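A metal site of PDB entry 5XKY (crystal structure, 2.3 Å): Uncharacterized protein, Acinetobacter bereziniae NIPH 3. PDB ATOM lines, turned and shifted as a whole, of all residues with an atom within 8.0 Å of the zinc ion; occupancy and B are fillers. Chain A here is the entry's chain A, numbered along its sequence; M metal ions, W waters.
The guanidinium group (NE) of Arg 361 lies within salt-bridge range of the side-chain carboxylate (OE2) of Glu 269, at 2.7 Å.
The side-chain carboxylate (OE2) of Glu 269 sits at hydrogen-bond distance from the indole nitrogen (NE1) of Trp 359 (2.8 Å).
O of Glu 269 sits at hydrogen-bond distance from N of Phe 332 (2.8 Å).
NE2 of His 265 sits close to NH2 of Arg 361, at 3.4 Å.
O of Pro 267 is in hydrogen-bond range of ND1 of His 265.
N of His 338 sits at hydrogen-bond distance from O of His 263, at 2.9 Å.
A ring nitrogen (ND1) of His 338 lies within hydrogen-bond range of the backbone carbonyl oxygen (O) of Ala 336.
A ring nitrogen (NE2) of His 263 sits close to the side-chain hydroxyl (OH) of Tyr 260 (3.4 Å).
Residues that only touch the zinc ion: His 263 (3.5 Å).
The nearest printed residue that does not touch the zinc ion is Arg 361 (4.4 Å).
The zinc ion is bound by OE1 of Glu 269 (2.1 Å), NE2 of His 265 (2.2 Å), NE2 of His 338 (2.3 Å), water W2 (2.4 Å) and water W1 (2.6 Å).
Water W1 bridges the side-chain hydroxyl of Tyr 271 (2.4 Å) and a ring nitrogen (NE2) of His 263 (3.0 Å).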
ATOM      1  N   TYR A 208     -27.259  37.600   4.433  1.00  0.00           N
ATOM      2  CA  TYR A 208     -27.774  37.694   3.062  1.00  0.00           C
ATOM      3  C   TYR A 208     -28.683  38.882   2.829  1.00  0.00           C
ATOM      4  O   TYR A 208     -29.165  39.066   1.692  1.00  0.00           O
ATOM      5  CB  TYR A 208     -28.520  36.405   2.678  1.00  0.00           C
ATOM      6  CG  TYR A 208     -27.576  35.243   2.486  1.00  0.00           C
ATOM      7  CD1 TYR A 208     -26.509  35.341   1.601  1.00  0.00           C
ATOM      8  CD2 TYR A 208     -27.716  34.064   3.214  1.00  0.00           C
ATOM      9  CE1 TYR A 208     -25.635  34.293   1.419  1.00  0.00           C
ATOM     10  CE2 TYR A 208     -26.838  33.003   3.034  1.00  0.00           C
ATOM     11  CZ  TYR A 208     -25.797  33.128   2.133  1.00  0.00           C
ATOM     12  OH  TYR A 208     -24.899  32.101   1.941  1.00  0.00           O
ATOM     13  N   TYR A 223     -32.614  35.082   7.440  1.00  0.00           N
ATOM     14  CA  TYR A 223     -31.446  34.282   7.742  1.00  0.00           C
ATOM     15  C   TYR A 223     -30.498  35.028   8.669  1.00  0.00           C
ATOM     16  O   TYR A 223     -30.321  36.245   8.546  1.00  0.00           O
ATOM     17  CB  TYR A 223     -30.701  33.836   6.446  1.00  0.00           C
ATOM     18  CG  TYR A 223     -29.567  32.888   6.767  1.00  0.00           C
ATOM     19  CD1 TYR A 223     -29.826  31.581   7.156  1.00  0.00           C
ATOM     20  CD2 TYR A 223     -28.232  33.300   6.745  1.00  0.00           C
ATOM     21  CE1 TYR A 223     -28.812  30.711   7.494  1.00  0.00           C
ATOM     22  CE2 TYR A 223     -27.209  32.443   7.048  1.00  0.00           C
ATOM     23  CZ  TYR A 223     -27.506  31.140   7.435  1.00  0.00           C
ATOM     24  OH  TYR A 223     -26.504  30.252   7.774  1.00  0.00           O
ATOM     25  N   TYR A 260     -33.256  28.165   1.325  1.00  0.00           N
ATOM     26  CA  TYR A 260     -31.863  28.566   1.183  1.00  0.00           C
ATOM     27  C   TYR A 260     -31.343  28.006  -0.141  1.00  0.00           C
ATOM     28  O   TYR A 260     -31.333  26.787  -0.311  1.00  0.00           O
ATOM     29  CB  TYR A 260     -31.060  28.045   2.363  1.00  0.00           C
ATOM     30  CG  TYR A 260     -29.627  28.556   2.554  1.00  0.00           C
ATOM     31  CD1 TYR A 260     -28.842  28.996   1.500  1.00  0.00           C
ATOM     32  CD2 TYR A 260     -29.069  28.560   3.829  1.00  0.00           C
ATOM     33  CE1 TYR A 260     -27.553  29.445   1.706  1.00  0.00           C
ATOM     34  CE2 TYR A 260     -27.779  28.982   4.055  1.00  0.00           C
ATOM     35  CZ  TYR A 260     -27.017  29.420   2.980  1.00  0.00           C
ATOM     36  OH  TYR A 260     -25.729  29.849   3.217  1.00  0.00           O
ATOM     37  N   HIS A 263     -25.955  25.980  -2.696  1.00  0.00           N
ATOM     38  CA  HIS A 263     -24.711  26.681  -2.440  1.00  0.00           C
ATOM     39  C   HIS A 263     -23.610  25.682  -2.082  1.00  0.00           C
ATOM     40  O   HIS A 263     -23.875  24.494  -1.813  1.00  0.00           O
ATOM     41  CB  HIS A 263     -24.893  27.769  -1.378  1.00  0.00           C
ATOM     42  CG  HIS A 263     -25.264  27.251  -0.014  1.00  0.00           C
ATOM     43  ND1 HIS A 263     -26.518  26.745   0.268  1.00  0.00           N
ATOM     44  CD2 HIS A 263     -24.566  27.209   1.147  1.00  0.00           C
ATOM     45  CE1 HIS A 263     -26.562  26.386   1.542  1.00  0.00           C
ATOM     46  NE2 HIS A 263     -25.392  26.663   2.101  1.00  0.00           N
ATOM     47  N   TYR A 264     -22.376  26.170  -2.100  1.00  0.00           N
ATOM     48  CA  TYR A 264     -21.185  25.335  -1.962  1.00  0.00           C
ATOM     49  C   TYR A 264     -20.019  26.238  -1.558  1.00  0.00           C
ATOM     50  O   TYR A 264     -20.092  27.467  -1.707  1.00  0.00           O
ATOM     51  CB  TYR A 264     -20.871  24.617  -3.287  1.00  0.00           C
ATOM     52  CG  TYR A 264     -20.685  25.622  -4.409  1.00  0.00           C
ATOM     53  CD1 TYR A 264     -21.785  26.187  -5.041  1.00  0.00           C
ATOM     54  CD2 TYR A 264     -19.417  26.015  -4.802  1.00  0.00           C
ATOM     55  CE1 TYR A 264     -21.627  27.144  -6.057  1.00  0.00           C
ATOM     56  CE2 TYR A 264     -19.240  26.948  -5.822  1.00  0.00           C
ATOM     57  CZ  TYR A 264     -20.351  27.511  -6.446  1.00  0.00           C
ATOM     58  OH  TYR A 264     -20.194  28.449  -7.431  1.00  0.00           O
ATOM     59  N   HIS A 265     -18.932  25.614  -1.073  1.00  0.00           N
ATOM     60  CA  HIS A 265     -17.714  26.342  -0.711  1.00  0.00           C
ATOM     61  C   HIS A 265     -16.571  25.361  -0.435  1.00  0.00           C
ATOM     62  O   HIS A 265     -16.799  24.175  -0.177  1.00  0.00           O
ATOM     63  CB  HIS A 265     -17.947  27.234   0.507  1.00  0.00           C
ATOM     64  CG  HIS A 265     -18.824  26.594   1.535  1.00  0.00           C
ATOM     65  ND1 HIS A 265     -18.379  25.575   2.351  1.00  0.00           N
ATOM     66  CD2 HIS A 265     -20.130  26.779   1.834  1.00  0.00           C
ATOM     67  CE1 HIS A 265     -19.368  25.192   3.138  1.00  0.00           C
ATOM     68  NE2 HIS A 265     -20.436  25.895   2.837  1.00  0.00           N
ATOM     69  N   PRO A 267     -14.492  25.191   2.346  1.00  0.00           N
ATOM     70  CA  PRO A 267     -14.346  24.591   3.682  1.00  0.00           C
ATOM     71  C   PRO A 267     -15.390  23.515   3.955  1.00  0.00           C
ATOM     72  O   PRO A 267     -16.569  23.679   3.636  1.00  0.00           O
ATOM     73  CB  PRO A 267     -14.500  25.786   4.631  1.00  0.00           C
ATOM     74  CG  PRO A 267     -15.233  26.807   3.867  1.00  0.00           C
ATOM     75  CD  PRO A 267     -14.834  26.635   2.428  1.00  0.00           C
ATOM     76  N   GLN A 268     -14.930  22.424   4.561  1.00  0.00           N
ATOM     77  CA  GLN A 268     -15.843  21.416   5.085  1.00  0.00           C
ATOM     78  C   GLN A 268     -16.709  22.005   6.193  1.00  0.00           C
ATOM     79  O   GLN A 268     -16.317  22.945   6.892  1.00  0.00           O
ATOM     80  CB  GLN A 268     -15.089  20.205   5.637  1.00  0.00           C
ATOM     81  CG  GLN A 268     -14.214  19.503   4.620  1.00  0.00           C
ATOM     82  CD  GLN A 268     -12.792  20.007   4.647  1.00  0.00           C
ATOM     83  OE1 GLN A 268     -12.536  21.224   4.769  1.00  0.00           O
ATOM     84  NE2 GLN A 268     -11.835  19.088   4.532  1.00  0.00           N
ATOM     85  N   GLU A 269     -17.896  21.417   6.371  1.00  0.00           N
ATOM     86  CA  GLU A 269     -18.897  22.018   7.230  1.00  0.00           C
ATOM     87  C   GLU A 269     -19.664  20.942   8.001  1.00  0.00           C
ATOM     88  O   GLU A 269     -19.838  19.816   7.515  1.00  0.00           O
ATOM     89  CB  GLU A 269     -19.841  22.874   6.408  1.00  0.00           C
ATOM     90  CG  GLU A 269     -20.428  24.009   7.177  1.00  0.00           C
ATOM     91  CD  GLU A 269     -21.024  25.032   6.274  1.00  0.00           C
ATOM     92  OE1 GLU A 269     -21.856  24.628   5.436  1.00  0.00           O
ATOM     93  OE2 GLU A 269     -20.656  26.214   6.382  1.00  0.00           O
ATOM     94  N   ILE A 270     -20.107  21.302   9.201  1.00  0.00           N
ATOM     95  CA  ILE A 270     -20.868  20.410  10.071  1.00  0.00           C
ATOM     96  C   ILE A 270     -22.114  21.146  10.554  1.00  0.00           C
ATOM     97  O   ILE A 270     -22.020  22.301  10.986  1.00  0.00           O
ATOM     98  CB  ILE A 270     -20.032  19.923  11.269  1.00  0.00           C
ATOM     99  CG1 ILE A 270     -18.708  19.310  10.819  1.00  0.00           C
ATOM    100  CG2 ILE A 270     -20.813  18.956  12.126  1.00  0.00           C
ATOM    101  CD1 ILE A 270     -17.712  19.115  11.958  1.00  0.00           C
ATOM    102  N   TYR A 271     -23.259  20.477  10.508  1.00  0.00           N
ATOM    103  CA  TYR A 271     -24.511  21.008  11.022  1.00  0.00           C
ATOM    104  C   TYR A 271     -25.108  20.031  12.022  1.00  0.00           C
ATOM    105  O   TYR A 271     -25.212  18.831  11.734  1.00  0.00           O
ATOM    106  CB  TYR A 271     -25.507  21.264   9.902  1.00  0.00           C
ATOM    107  CG  TYR A 271     -25.355  22.609   9.226  1.00  0.00           C
ATOM    108  CD1 TYR A 271     -26.012  23.736   9.722  1.00  0.00           C
ATOM    109  CD2 TYR A 271     -24.573  22.755   8.080  1.00  0.00           C
ATOM    110  CE1 TYR A 271     -25.904  24.963   9.111  1.00  0.00           C
ATOM    111  CE2 TYR A 271     -24.448  23.985   7.445  1.00  0.00           C
ATOM    112  CZ  TYR A 271     -25.122  25.088   7.972  1.00  0.00           C
ATOM    113  OH  TYR A 271     -25.010  26.302   7.362  1.00  0.00           O
ATOM    114  N   PHE A 332     -20.268  18.069   5.427  1.00  0.00           N
ATOM    115  CA  PHE A 332     -20.184  18.499   4.031  1.00  0.00           C
ATOM    116  C   PHE A 332     -18.726  18.455   3.603  1.00  0.00           C
ATOM    117  O   PHE A 332     -17.913  19.247   4.072  1.00  0.00           O
ATOM    118  CB  PHE A 332     -20.744  19.911   3.871  1.00  0.00           C
ATOM    119  CG  PHE A 332     -22.168  20.045   4.349  1.00  0.00           C
ATOM    120  CD1 PHE A 332     -22.465  20.051   5.699  1.00  0.00           C
ATOM    121  CD2 PHE A 332     -23.203  20.168   3.456  1.00  0.00           C
ATOM    122  CE1 PHE A 332     -23.770  20.172   6.141  1.00  0.00           C
ATOM    123  CE2 PHE A 332     -24.520  20.287   3.906  1.00  0.00           C
ATOM    124  CZ  PHE A 332     -24.797  20.287   5.220  1.00  0.00           C
ATOM    125  N   ALA A 336     -19.138  20.364  -1.542  1.00  0.00           N
ATOM    126  CA  ALA A 336     -20.387  19.620  -1.645  1.00  0.00           C
ATOM    127  C   ALA A 336     -21.533  20.609  -1.785  1.00  0.00           C
ATOM    128  O   ALA A 336     -21.580  21.647  -1.116  1.00  0.00           O
ATOM    129  CB  ALA A 336     -20.586  18.720  -0.423  1.00  0.00           C
ATOM    130  N   ILE A 337     -22.451  20.312  -2.699  1.00  0.00           N
ATOM    131  CA  ILE A 337     -23.580  21.204  -2.944  1.00  0.00           C
ATOM    132  C   ILE A 337     -24.661  20.911  -1.915  1.00  0.00           C
ATOM    133  O   ILE A 337     -24.969  19.748  -1.638  1.00  0.00           O
ATOM    134  CB  ILE A 337     -24.083  21.054  -4.394  1.00  0.00           C
ATOM    135  CG1 ILE A 337     -23.044  21.653  -5.367  1.00  0.00           C
ATOM    136  CG2 ILE A 337     -25.377  21.809  -4.576  1.00  0.00           C
ATOM    137  CD1 ILE A 337     -22.630  20.780  -6.437  1.00  0.00           C
ATOM    138  N   HIS A 338     -25.207  21.966  -1.308  1.00  0.00           N
ATOM    139  CA  HIS A 338     -26.227  21.773  -0.277  1.00  0.00           C
ATOM    140  C   HIS A 338     -27.283  22.866  -0.323  1.00  0.00           C
ATOM    141  O   HIS A 338     -27.129  23.895  -0.977  1.00  0.00           O
ATOM    142  CB  HIS A 338     -25.643  21.690   1.144  1.00  0.00           C
ATOM    143  CG  HIS A 338     -24.481  22.607   1.422  1.00  0.00           C
ATOM    144  ND1 HIS A 338     -23.277  22.506   0.770  1.00  0.00           N
ATOM    145  CD2 HIS A 338     -24.333  23.578   2.357  1.00  0.00           C
ATOM    146  CE1 HIS A 338     -22.441  23.405   1.266  1.00  0.00           C
ATOM    147  NE2 HIS A 338     -23.056  24.064   2.226  1.00  0.00           N
ATOM    148  N   ALA A 339     -28.392  22.585   0.374  1.00  0.00           N
ATOM    149  CA  ALA A 339     -29.549  23.467   0.421  1.00  0.00           C
ATOM    150  C   ALA A 339     -30.363  23.166   1.661  1.00  0.00           C
ATOM    151  O   ALA A 339     -30.335  22.050   2.186  1.00  0.00           O
ATOM    152  CB  ALA A 339     -30.418  23.313  -0.839  1.00  0.00           C
ATOM    153  N   PHE A 340     -31.082  24.177   2.147  1.00  0.00           N
ATOM    154  CA  PHE A 340     -31.923  24.049   3.338  1.00  0.00           C
ATOM    155  C   PHE A 340     -33.298  24.590   2.992  1.00  0.00           C
ATOM    156  O   PHE A 340     -33.441  25.770   2.670  1.00  0.00           O
ATOM    157  CB  PHE A 340     -31.325  24.798   4.541  1.00  0.00           C
ATOM    158  CG  PHE A 340     -30.000  24.261   4.980  1.00  0.00           C
ATOM    159  CD1 PHE A 340     -29.921  23.052   5.661  1.00  0.00           C
ATOM    160  CD2 PHE A 340     -28.831  24.933   4.677  1.00  0.00           C
ATOM    161  CE1 PHE A 340     -28.704  22.537   6.052  1.00  0.00           C
ATOM    162  CE2 PHE A 340     -27.603  24.420   5.060  1.00  0.00           C
ATOM    163  CZ  PHE A 340     -27.534  23.224   5.756  1.00  0.00           C
ATOM    164  N   TRP A 359     -23.587  25.208  14.172  1.00  0.00           N
ATOM    165  CA  TRP A 359     -22.914  25.253  12.882  1.00  0.00           C
ATOM    166  C   TRP A 359     -21.412  25.305  13.097  1.00  0.00           C
ATOM    167  O   TRP A 359     -20.921  25.905  14.058  1.00  0.00           O
ATOM    168  CB  TRP A 359     -23.395  26.460  12.057  1.00  0.00           C
ATOM    169  CG  TRP A 359     -22.477  26.899  10.978  1.00  0.00           C
ATOM    170  CD1 TRP A 359     -22.411  26.410   9.694  1.00  0.00           C
ATOM    171  CD2 TRP A 359     -21.507  27.936  11.061  1.00  0.00           C
ATOM    172  NE1 TRP A 359     -21.426  27.089   8.978  1.00  0.00           N
ATOM    173  CE2 TRP A 359     -20.870  28.041   9.800  1.00  0.00           C
ATOM    174  CE3 TRP A 359     -21.116  28.817  12.074  1.00  0.00           C
ATOM    175  CZ2 TRP A 359     -19.874  28.971   9.542  1.00  0.00           C
ATOM    176  CZ3 TRP A 359     -20.120  29.747  11.816  1.00  0.00           C
ATOM    177  CH2 TRP A 359     -19.501  29.810  10.555  1.00  0.00           C
ATOM    178  N   ALA A 360     -20.682  24.663  12.193  1.00  0.00           N
ATOM    179  CA  ALA A 360     -19.232  24.666  12.309  1.00  0.00           C
ATOM    180  C   ALA A 360     -18.605  24.437  10.949  1.00  0.00           C
ATOM    181  O   ALA A 360     -19.185  23.791  10.072  1.00  0.00           O
ATOM    182  CB  ALA A 360     -18.767  23.599  13.287  1.00  0.00           C
ATOM    183  N   ARG A 361     -17.395  24.969  10.798  1.00  0.00           N
ATOM    184  CA  ARG A 361     -16.500  24.627   9.706  1.00  0.00           C
ATOM    185  C   ARG A 361     -15.178  24.144  10.290  1.00  0.00           C
ATOM    186  O   ARG A 361     -14.782  24.575  11.378  1.00  0.00           O
ATOM    187  CB  ARG A 361     -16.292  25.824   8.768  1.00  0.00           C
ATOM    188  CG  ARG A 361     -17.508  26.150   7.905  1.00  0.00           C
ATOM    189  CD  ARG A 361     -17.313  27.450   7.128  1.00  0.00           C
ATOM    190  NE  ARG A 361     -18.361  27.638   6.124  1.00  0.00           N
ATOM    191  CZ  ARG A 361     -18.403  28.659   5.268  1.00  0.00           C
ATOM    192  NH1 ARG A 361     -17.453  29.601   5.282  1.00  0.00           N
ATOM    193  NH2 ARG A 361     -19.387  28.730   4.369  1.00  0.00           N
ATOM    194  N   THR A 371     -18.695  31.634   0.861  1.00  0.00           N
ATOM    195  CA  THR A 371     -19.902  30.870   0.552  1.00  0.00           C
ATOM    196  C   THR A 371     -20.414  31.261  -0.826  1.00  0.00           C
ATOM    197  O   THR A 371     -20.883  32.383  -1.017  1.00  0.00           O
ATOM    198  CB  THR A 371     -20.973  31.133   1.611  1.00  0.00           C
ATOM    199  OG1 THR A 371     -20.464  30.754   2.901  1.00  0.00           O
ATOM    200  CG2 THR A 371     -22.226  30.321   1.310  1.00  0.00           C
ATOM    201  N   GLN A 372     -20.341  30.338  -1.783  1.00  0.00           N
ATOM    202  CA  GLN A 372     -20.773  30.598  -3.148  1.00  0.00           C
ATOM    203  C   GLN A 372     -22.232  30.199  -3.320  1.00  0.00           C
ATOM    204  O   GLN A 372     -22.648  29.119  -2.887  1.00  0.00           O
ATOM    205  CB  GLN A 372     -19.941  29.817  -4.162  1.00  0.00           C
ATOM    206  CG  GLN A 372     -18.434  29.850  -3.932  1.00  0.00           C
ATOM    207  CD  GLN A 372     -17.806  31.173  -4.344  1.00  0.00           C
ATOM    208  OE1 GLN A 372     -18.504  32.153  -4.613  1.00  0.00           O
ATOM    209  NE2 GLN A 372     -16.478  31.201  -4.402  1.00  0.00           N
HETATM  210 ZN    ZN M   1     -22.449  25.682   3.720  1.00  0.00          ZN
HETATM  211  O   HOH W   1     -24.502  26.519   4.992  1.00  0.00           O
HETATM  212  O   HOH W   2     -22.808  27.920   4.343  1.00  0.00           O
